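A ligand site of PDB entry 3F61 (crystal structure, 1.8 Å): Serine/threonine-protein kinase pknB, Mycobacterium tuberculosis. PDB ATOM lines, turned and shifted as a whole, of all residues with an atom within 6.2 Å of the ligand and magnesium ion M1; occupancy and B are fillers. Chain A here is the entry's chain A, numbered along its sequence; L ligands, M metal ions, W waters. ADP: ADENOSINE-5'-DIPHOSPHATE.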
ATOM      1  N   LEU A  20       9.025 -26.997  -3.197  1.00  0.00           N
ATOM      2  CA  LEU A  20       9.168 -25.582  -3.458  1.00  0.00           C
ATOM      3  C   LEU A  20       7.886 -24.928  -3.999  1.00  0.00           C
ATOM      4  O   LEU A  20       7.626 -23.753  -3.786  1.00  0.00           O
ATOM      5  CB  LEU A  20      10.290 -25.395  -4.479  1.00  0.00           C
ATOM      6  CG  LEU A  20      11.662 -25.830  -3.999  1.00  0.00           C
ATOM      7  CD1 LEU A  20      12.641 -25.708  -5.140  1.00  0.00           C
ATOM      8  CD2 LEU A  20      12.121 -24.947  -2.803  1.00  0.00           C
ATOM      9  N   GLY A  21       7.058 -25.702  -4.696  1.00  0.00           N
ATOM     10  CA  GLY A  21       5.927 -25.100  -5.385  1.00  0.00           C
ATOM     11  C   GLY A  21       5.146 -26.155  -6.156  1.00  0.00           C
ATOM     12  O   GLY A  21       5.558 -27.313  -6.194  1.00  0.00           O
ATOM     13  N   PHE A  22       4.007 -25.756  -6.703  1.00  0.00           N
ATOM     14  CA  PHE A  22       3.209 -26.667  -7.552  1.00  0.00           C
ATOM     15  C   PHE A  22       2.439 -25.859  -8.541  1.00  0.00           C
ATOM     16  O   PHE A  22       2.243 -24.660  -8.356  1.00  0.00           O
ATOM     17  CB  PHE A  22       2.208 -27.504  -6.737  1.00  0.00           C
ATOM     18  CG  PHE A  22       1.086 -26.673  -6.120  1.00  0.00           C
ATOM     19  CD1 PHE A  22      -0.171 -26.577  -6.747  1.00  0.00           C
ATOM     20  CD2 PHE A  22       1.322 -25.966  -4.944  1.00  0.00           C
ATOM     21  CE1 PHE A  22      -1.177 -25.770  -6.197  1.00  0.00           C
ATOM     22  CE2 PHE A  22       0.308 -25.162  -4.382  1.00  0.00           C
ATOM     23  CZ  PHE A  22      -0.946 -25.072  -5.019  1.00  0.00           C
ATOM     24  N   GLY A  23       1.958 -26.522  -9.584  1.00  0.00           N
ATOM     25  CA  GLY A  23       1.070 -25.911 -10.533  1.00  0.00           C
ATOM     26  C   GLY A  23      -0.017 -26.923 -10.877  1.00  0.00           C
ATOM     27  O   GLY A  23      -0.294 -27.844 -10.117  1.00  0.00           O
ATOM     28  N   GLY A  24      -0.637 -26.719 -12.029  1.00  0.00           N
ATOM     29  CA  GLY A  24      -1.794 -27.509 -12.430  1.00  0.00           C
ATOM     30  C   GLY A  24      -1.392 -28.902 -12.853  1.00  0.00           C
ATOM     31  O   GLY A  24      -2.247 -29.779 -12.968  1.00  0.00           O
ATOM     32  N   MET A  25      -0.096 -29.134 -13.063  1.00  0.00           N
ATOM     33  CA  MET A  25       0.352 -30.462 -13.497  1.00  0.00           C
ATOM     34  C   MET A  25       1.495 -31.010 -12.642  1.00  0.00           C
ATOM     35  O   MET A  25       1.632 -32.204 -12.512  1.00  0.00           O
ATOM     36  CB  MET A  25       0.775 -30.427 -14.992  1.00  0.00           C
ATOM     37  CG  MET A  25       1.401 -31.727 -15.479  1.00  0.00           C
ATOM     38  SD  MET A  25       1.583 -31.681 -17.292  1.00  0.00           S
ATOM     39  CE  MET A  25       2.857 -30.444 -17.464  1.00  0.00           C
ATOM     40  N   SER A  26       2.331 -30.132 -12.052  1.00  0.00           N
ATOM     41  CA  SER A  26       3.632 -30.570 -11.534  1.00  0.00           C
ATOM     42  C   SER A  26       3.843 -30.126 -10.104  1.00  0.00           C
ATOM     43  O   SER A  26       3.199 -29.151  -9.651  1.00  0.00           O
ATOM     44  CB  SER A  26       4.765 -29.949 -12.371  1.00  0.00           C
ATOM     45  OG  SER A  26       4.637 -30.311 -13.737  1.00  0.00           O
ATOM     46  N   GLU A  27       4.755 -30.812  -9.416  1.00  0.00           N
ATOM     47  CA  GLU A  27       5.284 -30.337  -8.127  1.00  0.00           C
ATOM     48  C   GLU A  27       6.736 -30.058  -8.364  1.00  0.00           C
ATOM     49  O   GLU A  27       7.398 -30.772  -9.122  1.00  0.00           O
ATOM     50  CB  GLU A  27       5.232 -31.403  -7.036  1.00  0.00           C
ATOM     51  CG  GLU A  27       4.327 -32.524  -7.326  1.00  0.00           C
ATOM     52  CD  GLU A  27       4.175 -33.529  -6.209  1.00  0.00           C
ATOM     53  OE1 GLU A  27       3.079 -34.093  -6.130  1.00  0.00           O
ATOM     54  OE2 GLU A  27       5.132 -33.809  -5.454  1.00  0.00           O
ATOM     55  N   VAL A  28       7.250 -29.028  -7.682  1.00  0.00           N
ATOM     56  CA  VAL A  28       8.658 -28.700  -7.831  1.00  0.00           C
ATOM     57  C   VAL A  28       9.356 -28.823  -6.459  1.00  0.00           C
ATOM     58  O   VAL A  28       8.927 -28.218  -5.461  1.00  0.00           O
ATOM     59  CB  VAL A  28       8.845 -27.302  -8.430  1.00  0.00           C
ATOM     60  CG1 VAL A  28      10.352 -27.000  -8.578  1.00  0.00           C
ATOM     61  CG2 VAL A  28       8.147 -27.197  -9.816  1.00  0.00           C
ATOM     62  N   ALA A  41      16.382 -27.902  -8.828  1.00  0.00           N
ATOM     63  CA  ALA A  41      14.917 -28.011  -8.657  1.00  0.00           C
ATOM     64  C   ALA A  41      14.451 -29.133  -9.571  1.00  0.00           C
ATOM     65  O   ALA A  41      14.844 -29.181 -10.738  1.00  0.00           O
ATOM     66  CB  ALA A  41      14.224 -26.713  -9.026  1.00  0.00           C
ATOM     67  N   LYS A  43      11.239 -30.802 -11.218  1.00  0.00           N
ATOM     68  CA  LYS A  43       9.837 -30.670 -11.530  1.00  0.00           C
ATOM     69  C   LYS A  43       9.318 -32.083 -11.845  1.00  0.00           C
ATOM     70  O   LYS A  43       9.806 -32.712 -12.772  1.00  0.00           O
ATOM     71  CB  LYS A  43       9.646 -29.711 -12.725  1.00  0.00           C
ATOM     72  CG  LYS A  43       8.229 -29.717 -13.299  1.00  0.00           C
ATOM     73  CD  LYS A  43       8.056 -28.741 -14.450  1.00  0.00           C
ATOM     74  CE  LYS A  43       8.099 -27.303 -13.913  1.00  0.00           C
ATOM     75  NZ  LYS A  43       7.688 -26.322 -14.990  1.00  0.00           N
ATOM     76  N   VAL A  75      16.198 -19.598 -16.173  1.00  0.00           N
ATOM     77  CA  VAL A  75      16.391 -20.883 -15.488  1.00  0.00           C
ATOM     78  C   VAL A  75      16.878 -21.933 -16.482  1.00  0.00           C
ATOM     79  O   VAL A  75      16.147 -22.283 -17.443  1.00  0.00           O
ATOM     80  CB  VAL A  75      15.055 -21.337 -14.818  1.00  0.00           C
ATOM     81  CG1 VAL A  75      15.148 -22.753 -14.222  1.00  0.00           C
ATOM     82  CG2 VAL A  75      14.676 -20.307 -13.726  1.00  0.00           C
ATOM     83  N   MET A  95      16.152 -28.867 -13.208  1.00  0.00           N
ATOM     84  CA  MET A  95      16.533 -27.546 -13.648  1.00  0.00           C
ATOM     85  C   MET A  95      17.268 -26.775 -12.582  1.00  0.00           C
ATOM     86  O   MET A  95      17.388 -27.194 -11.426  1.00  0.00           O
ATOM     87  CB  MET A  95      15.301 -26.773 -14.084  1.00  0.00           C
ATOM     88  CG  MET A  95      14.327 -26.568 -12.989  1.00  0.00           C
ATOM     89  SD  MET A  95      12.689 -26.015 -13.543  1.00  0.00           S
ATOM     90  CE  MET A  95      11.883 -27.520 -13.962  1.00  0.00           C
ATOM     91  N   GLU A  96      17.731 -25.609 -12.999  1.00  0.00           N
ATOM     92  CA  GLU A  96      18.350 -24.641 -12.100  1.00  0.00           C
ATOM     93  C   GLU A  96      17.396 -24.277 -10.947  1.00  0.00           C
ATOM     94  O   GLU A  96      16.225 -23.895 -11.157  1.00  0.00           O
ATOM     95  CB  GLU A  96      18.737 -23.410 -12.908  1.00  0.00           C
ATOM     96  CG  GLU A  96      19.314 -22.338 -12.072  1.00  0.00           C
ATOM     97  CD  GLU A  96      19.646 -21.083 -12.876  1.00  0.00           C
ATOM     98  OE1 GLU A  96      19.825 -20.043 -12.205  1.00  0.00           O
ATOM     99  OE2 GLU A  96      19.739 -21.124 -14.137  1.00  0.00           O
ATOM    100  N   TYR A  97      17.898 -24.391  -9.719  1.00  0.00           N
ATOM    101  CA  TYR A  97      17.147 -24.035  -8.539  1.00  0.00           C
ATOM    102  C   TYR A  97      17.242 -22.531  -8.338  1.00  0.00           C
ATOM    103  O   TYR A  97      18.355 -21.969  -8.362  1.00  0.00           O
ATOM    104  CB  TYR A  97      17.762 -24.747  -7.322  1.00  0.00           C
ATOM    105  CG  TYR A  97      17.385 -24.191  -5.964  1.00  0.00           C
ATOM    106  CD1 TYR A  97      18.372 -23.822  -5.048  1.00  0.00           C
ATOM    107  CD2 TYR A  97      16.051 -24.089  -5.571  1.00  0.00           C
ATOM    108  CE1 TYR A  97      18.037 -23.327  -3.785  1.00  0.00           C
ATOM    109  CE2 TYR A  97      15.702 -23.593  -4.325  1.00  0.00           C
ATOM    110  CZ  TYR A  97      16.707 -23.223  -3.440  1.00  0.00           C
ATOM    111  OH  TYR A  97      16.359 -22.751  -2.192  1.00  0.00           O
ATOM    112  N   VAL A  98      16.094 -21.898  -8.133  1.00  0.00           N
ATOM    113  CA  VAL A  98      16.015 -20.513  -7.679  1.00  0.00           C
ATOM    114  C   VAL A  98      15.492 -20.471  -6.251  1.00  0.00           C
ATOM    115  O   VAL A  98      14.406 -20.970  -5.977  1.00  0.00           O
ATOM    116  CB  VAL A  98      15.068 -19.685  -8.583  1.00  0.00           C
ATOM    117  CG1 VAL A  98      14.990 -18.227  -8.099  1.00  0.00           C
ATOM    118  CG2 VAL A  98      15.543 -19.737 -10.021  1.00  0.00           C
ATOM    119  N   ASP A  99      16.277 -19.891  -5.346  1.00  0.00           N
ATOM    120  CA  ASP A  99      15.829 -19.648  -3.985  1.00  0.00           C
ATOM    121  C   ASP A  99      15.184 -18.281  -4.051  1.00  0.00           C
ATOM    122  O   ASP A  99      15.897 -17.281  -4.214  1.00  0.00           O
ATOM    123  CB  ASP A  99      17.041 -19.611  -3.040  1.00  0.00           C
ATOM    124  CG  ASP A  99      16.665 -19.278  -1.612  1.00  0.00           C
ATOM    125  OD1 ASP A  99      15.467 -19.193  -1.295  1.00  0.00           O
ATOM    126  OD2 ASP A  99      17.603 -19.094  -0.809  1.00  0.00           O
ATOM    127  N   GLY A 100      13.862 -18.231  -4.010  1.00  0.00           N
ATOM    128  CA  GLY A 100      13.167 -16.965  -4.167  1.00  0.00           C
ATOM    129  C   GLY A 100      11.663 -17.098  -4.262  1.00  0.00           C
ATOM    130  O   GLY A 100      11.084 -18.056  -3.752  1.00  0.00           O
ATOM    131  N   THR A 102       8.001 -16.314  -6.835  1.00  0.00           N
ATOM    132  CA  THR A 102       7.505 -15.925  -8.150  1.00  0.00           C
ATOM    133  C   THR A 102       6.786 -14.578  -8.060  1.00  0.00           C
ATOM    134  O   THR A 102       6.392 -14.172  -6.971  1.00  0.00           O
ATOM    135  CB  THR A 102       6.485 -16.931  -8.728  1.00  0.00           C
ATOM    136  OG1 THR A 102       5.277 -16.883  -7.959  1.00  0.00           O
ATOM    137  CG2 THR A 102       7.059 -18.356  -8.773  1.00  0.00           C
ATOM    138  N   ARG A 104       3.831 -14.147  -9.063  1.00  0.00           N
ATOM    139  CA  ARG A 104       2.537 -14.562  -8.583  1.00  0.00           C
ATOM    140  C   ARG A 104       2.515 -14.566  -7.054  1.00  0.00           C
ATOM    141  O   ARG A 104       1.544 -14.073  -6.453  1.00  0.00           O
ATOM    142  CB  ARG A 104       2.247 -15.960  -9.069  1.00  0.00           C
ATOM    143  CG  ARG A 104       0.900 -16.460  -8.643  1.00  0.00           C
ATOM    144  CD  ARG A 104       0.583 -17.762  -9.352  1.00  0.00           C
ATOM    145  NE  ARG A 104      -0.758 -18.212  -9.048  1.00  0.00           N
ATOM    146  CZ  ARG A 104      -1.029 -19.142  -8.136  1.00  0.00           C
ATOM    147  NH1 ARG A 104      -0.049 -19.700  -7.452  1.00  0.00           N
ATOM    148  NH2 ARG A 104      -2.281 -19.515  -7.908  1.00  0.00           N
ATOM    149  N   ASP A 105       3.568 -15.132  -6.437  1.00  0.00           N
ATOM    150  CA  ASP A 105       3.711 -15.137  -4.960  1.00  0.00           C
ATOM    151  C   ASP A 105       3.693 -13.696  -4.422  1.00  0.00           C
ATOM    152  O   ASP A 105       2.945 -13.362  -3.495  1.00  0.00           O
ATOM    153  CB  ASP A 105       5.034 -15.803  -4.519  1.00  0.00           C
ATOM    154  CG  ASP A 105       5.085 -17.347  -4.744  1.00  0.00           C
ATOM    155  OD1 ASP A 105       6.225 -17.895  -4.833  1.00  0.00           O
ATOM    156  OD2 ASP A 105       4.019 -17.980  -4.831  1.00  0.00           O
ATOM    157  N   ASP A 141       4.452 -18.756 -22.770  1.00  0.00           N
ATOM    158  CA  ASP A 141       3.675 -18.884 -21.534  1.00  0.00           C
ATOM    159  C   ASP A 141       4.184 -17.874 -20.480  1.00  0.00           C
ATOM    160  O   ASP A 141       4.358 -18.213 -19.316  1.00  0.00           O
ATOM    161  CB  ASP A 141       3.776 -20.337 -21.023  1.00  0.00           C
ATOM    162  CG  ASP A 141       2.842 -20.640 -19.858  1.00  0.00           C
ATOM    163  OD1 ASP A 141       3.216 -21.522 -19.045  1.00  0.00           O
ATOM    164  OD2 ASP A 141       1.758 -20.023 -19.754  1.00  0.00           O
ATOM    165  N   LYS A 143       3.919 -15.430 -17.750  1.00  0.00           N
ATOM    166  CA  LYS A 143       2.887 -15.249 -16.722  1.00  0.00           C
ATOM    167  C   LYS A 143       3.619 -15.064 -15.398  1.00  0.00           C
ATOM    168  O   LYS A 143       4.831 -15.373 -15.288  1.00  0.00           O
ATOM    169  CB  LYS A 143       1.918 -16.454 -16.646  1.00  0.00           C
ATOM    170  CG  LYS A 143       2.601 -17.769 -16.272  1.00  0.00           C
ATOM    171  CD  LYS A 143       1.663 -18.973 -16.440  1.00  0.00           C
ATOM    172  CE  LYS A 143       2.267 -20.216 -15.772  1.00  0.00           C
ATOM    173  NZ  LYS A 143       1.374 -21.389 -16.016  1.00  0.00           N
ATOM    174  N   ALA A 145       3.741 -16.722 -12.585  1.00  0.00           N
ATOM    175  CA  ALA A 145       4.400 -17.876 -11.950  1.00  0.00           C
ATOM    176  C   ALA A 145       5.683 -18.327 -12.675  1.00  0.00           C
ATOM    177  O   ALA A 145       6.459 -19.148 -12.148  1.00  0.00           O
ATOM    178  CB  ALA A 145       3.465 -19.057 -11.853  1.00  0.00           C
ATOM    179  N   ASN A 146       5.887 -17.840 -13.894  1.00  0.00           N
ATOM    180  CA  ASN A 146       7.086 -18.149 -14.647  1.00  0.00           C
ATOM    181  C   ASN A 146       8.204 -17.118 -14.533  1.00  0.00           C
ATOM    182  O   ASN A 146       9.201 -17.162 -15.255  1.00  0.00           O
ATOM    183  CB  ASN A 146       6.753 -18.462 -16.134  1.00  0.00           C
ATOM    184  CG  ASN A 146       6.204 -19.890 -16.305  1.00  0.00           C
ATOM    185  OD1 ASN A 146       6.471 -20.755 -15.466  1.00  0.00           O
ATOM    186  ND2 ASN A 146       5.423 -20.137 -17.379  1.00  0.00           N
ATOM    187  N   MET A 148      10.630 -15.352 -11.494  1.00  0.00           N
ATOM    188  CA  MET A 148      10.963 -15.337 -10.074  1.00  0.00           C
ATOM    189  C   MET A 148      11.972 -14.241  -9.770  1.00  0.00           C
ATOM    190  O   MET A 148      12.750 -13.825 -10.631  1.00  0.00           O
ATOM    191  CB  MET A 148      11.515 -16.683  -9.605  1.00  0.00           C
ATOM    192  CG  MET A 148      10.450 -17.807  -9.476  1.00  0.00           C
ATOM    193  SD  MET A 148      11.193 -19.369  -8.961  1.00  0.00           S
ATOM    194  CE  MET A 148      11.270 -19.169  -7.180  1.00  0.00           C
ATOM    195  N   MET A 158      11.473 -18.579 -16.552  1.00  0.00           N
ATOM    196  CA  MET A 158      11.576 -20.008 -16.742  1.00  0.00           C
ATOM    197  C   MET A 158      10.451 -20.587 -17.594  1.00  0.00           C
ATOM    198  O   MET A 158       9.459 -19.895 -17.866  1.00  0.00           O
ATOM    199  CB  MET A 158      11.608 -20.704 -15.381  1.00  0.00           C
ATOM    200  CG  MET A 158      10.281 -20.599 -14.661  1.00  0.00           C
ATOM    201  SD  MET A 158      10.555 -20.947 -12.915  1.00  0.00           S
ATOM    202  CE  MET A 158      11.241 -19.371 -12.410  1.00  0.00           C
ATOM    203  N   ASP A 159      10.636 -21.838 -18.006  1.00  0.00           N
ATOM    204  CA  ASP A 159       9.604 -22.628 -18.727  1.00  0.00           C
ATOM    205  C   ASP A 159       9.288 -22.063 -20.096  1.00  0.00           C
ATOM    206  O   ASP A 159       8.140 -21.731 -20.402  1.00  0.00           O
ATOM    207  CB  ASP A 159       8.333 -22.802 -17.861  1.00  0.00           C
ATOM    208  CG  ASP A 159       8.636 -23.524 -16.538  1.00  0.00           C
ATOM    209  OD1 ASP A 159       9.614 -24.305 -16.496  1.00  0.00           O
ATOM    210  OD2 ASP A 159       7.887 -23.339 -15.548  1.00  0.00           O
HETATM  211  PB  ADP L   1       3.262 -22.905 -13.339  1.00  0.00           P
HETATM  212  O1B ADP L   1       4.448 -22.008 -13.606  1.00  0.00           O
HETATM  213  O2B ADP L   1       2.177 -22.363 -12.467  1.00  0.00           O
HETATM  214  O3B ADP L   1       2.718 -23.440 -14.647  1.00  0.00           O
HETATM  215  PA  ADP L   1       5.171 -24.989 -12.664  1.00  0.00           P
HETATM  216  O1A ADP L   1       4.952 -26.463 -12.527  1.00  0.00           O
HETATM  217  O2A ADP L   1       6.009 -24.499 -13.826  1.00  0.00           O
HETATM  218  O3A ADP L   1       3.760 -24.226 -12.528  1.00  0.00           O
HETATM  219  O5' ADP L   1       5.911 -24.501 -11.346  1.00  0.00           O
HETATM  220  C5' ADP L   1       5.184 -24.641 -10.122  1.00  0.00           C
HETATM  221  C4' ADP L   1       5.782 -23.741  -9.045  1.00  0.00           C
HETATM  222  O4' ADP L   1       7.037 -24.276  -8.668  1.00  0.00           O
HETATM  223  C3' ADP L   1       6.143 -22.364  -9.537  1.00  0.00           C
HETATM  224  O3' ADP L   1       5.063 -21.431  -9.508  1.00  0.00           O
HETATM  225  C2' ADP L   1       7.197 -21.930  -8.563  1.00  0.00           C
HETATM  226  O2' ADP L   1       6.578 -21.616  -7.303  1.00  0.00           O
HETATM  227  C1' ADP L   1       7.949 -23.223  -8.311  1.00  0.00           C
HETATM  228  N9  ADP L   1       9.116 -23.342  -9.210  1.00  0.00           N
HETATM  229  C8  ADP L   1       9.078 -23.679 -10.523  1.00  0.00           C
HETATM  230  N7  ADP L   1      10.341 -23.735 -11.015  1.00  0.00           N
HETATM  231  C5  ADP L   1      11.206 -23.411 -10.029  1.00  0.00           C
HETATM  232  C6  ADP L   1      12.683 -23.270  -9.924  1.00  0.00           C
HETATM  233  N6  ADP L   1      13.466 -23.520 -10.998  1.00  0.00           N
HETATM  234  N1  ADP L   1      13.186 -22.923  -8.725  1.00  0.00           N
HETATM  235  C2  ADP L   1      12.370 -22.728  -7.655  1.00  0.00           C
HETATM  236  N3  ADP L   1      11.004 -22.808  -7.673  1.00  0.00           N
HETATM  237  C4  ADP L   1      10.391 -23.159  -8.836  1.00  0.00           C
HETATM  238 MG    MG M   1       6.221 -22.668 -14.622  1.00  0.00          MG
HETATM  239 MG    MG M   2       2.383 -27.307 -12.954  1.00  0.00          MG
HETATM  240 MG    MG M   3       0.706 -17.209 -13.016  1.00  0.00          MG
HETATM  241  O   HOH W   1      -0.150 -23.892 -12.916  1.00  0.00           O
HETATM  242  O   HOH W   2      10.189 -21.728  -5.214  1.00  0.00           O
HETATM  243  O   HOH W   3       7.781 -20.409  -5.524  1.00  0.00           O
HETATM  244  O   HOH W   4       7.407 -21.805 -12.998  1.00  0.00           O
HETATM  245  O   HOH W   5       9.856 -24.511 -13.648  1.00  0.00           O
HETATM  246  O   HOH W   6       2.225 -22.049  -9.989  1.00  0.00           O
HETATM  247  O   HOH W   7       5.056 -23.142 -16.298  1.00  0.00           O
HETATM  248  O   HOH W   8       4.769 -27.892 -15.363  1.00  0.00           O
HETATM  249  O   HOH W   9       0.101 -20.190 -12.984  1.00  0.00           O
HETATM  250  O   HOH W  10       1.942 -26.029 -15.326  1.00  0.00           O
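Magnesium ion M1 is bound by an oxygen (O2A) of the ligand (2.0 Å), the side-chain carboxylate (OD2) of Asp 159 (2.0 Å), water W7 (2.1 Å), the side-chain amide oxygen (OD1) of Asn 146 (2.1 Å), an oxygen (O1B) of the ligand (2.1 Å) and water W4 (2.2 Å). Magnesium ion M1 has six donor atoms within binding distance.
The side-chain sulfur (SD) of Met 95 is in hydrogen-bond range of a nitrogen (N6) of the ligand (3.6 Å). NZ of Lys 43 is in salt-bridge range of O1A of the ligand, 3.7 Å away. A nitrogen (N6) of the ligand lies within hydrogen-bond range of the backbone carbonyl oxygen of Glu 96 (2.8 Å). The side-chain amino group of Lys 143 lies within salt-bridge range of an oxygen (O3B) of the ligand (2.8 Å). A nitrogen (N1) of the ligand lies within hydrogen-bond range of the backbone NH (N) of Val 98 (3.1 Å).
N3 of the ligand sits close to SD of Met 148 (3.7 Å). SD of Met 158 sits close to N7 of the ligand. CD1 of Leu 20 touches C2 of the ligand, at 3.9 Å. Gly 21 touches the ligand (CA to O4', 3.6 Å). C of Phe 22 touches C5' of the ligand, at 3.4 Å. Gly 23 touches the ligand. Ser 26 touches the ligand (CB to O1A, 3.5 Å). Val 28 touches the ligand (CG2 to O4', 3.3 Å). Ala 41 touches the ligand (CB to N6, 3.8 Å). CG1 of Val 75 touches N6 of the ligand, 3.7 Å away. CG2 of Thr 102 touches C2' of the ligand (3.6 Å). Ala 145 touches the ligand. Of the 28 residues printed, 19 come within 4 Å of the ligand. The nearest printed residue that does not touch the ligand is Tyr 97 (4.1 Å).
Water W7 lies within hydrogen-bond range of an oxygen (O3B) of the ligand (2.9 Å) and the side-chain amide nitrogen of Asn 146 (3.2 Å). Water W3 bridges an oxygen (O2') of the ligand and the side-chain carboxylate (OD1) of Asp 105. Water W6 lies within hydrogen-bond range of an oxygen (O2B) of the ligand (2.5 Å) and the backbone carbonyl oxygen of Phe 22 (3.1 Å). Water W1 lies within hydrogen-bond range of O2B of the ligand and N of Gly 24. Water W8 lies within hydrogen-bond range of the side-chain hydroxyl of Ser 26 (2.9 Å), an oxygen (O1A) of the ligand (3.2 Å) and the side-chain amino group of Lys 43 (3.3 Å).
Residues that only touch magnesium ion M1: Lys 43 (3.95 Å). Three residues have an atom within 4 Å of magnesium ion M1: Lys 43, Asn 146 and Asp 159. The nearest printed residue that does not touch magnesium ion M1 is Ala 145 (4.3 Å).
ND2 of Asn 146 lies within hydrogen-bond range of O of Asp 141, 2.9 Å away. The backbone NH (N) of Val 28 lies within hydrogen-bond range of the backbone carbonyl oxygen (O) of Gly 21, 2.8 Å away. The backbone carbonyl oxygen (O) of Asn 146 sits at hydrogen-bond distance from the backbone NH (N) of Met 158 (3.0 Å). N of Leu 20 is in hydrogen-bond range of O of Val 28 (2.6 Å). The backbone NH of Met 95 sits at hydrogen-bond distance from the backbone carbonyl oxygen of Ala 41 (2.8 Å). OD1 of Asp 159 is in salt-bridge range of NZ of Lys 43, at 3.2 Å. The side-chain amino group (NZ) of Lys 143 is in salt-bridge range of the side-chain carboxylate (OD1) of Asp 141 (3.5 Å). The backbone NH (N) of Asp 105 sits at hydrogen-bond distance from the side-chain hydroxyl (OG1) of Thr 102 (2.9 Å).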
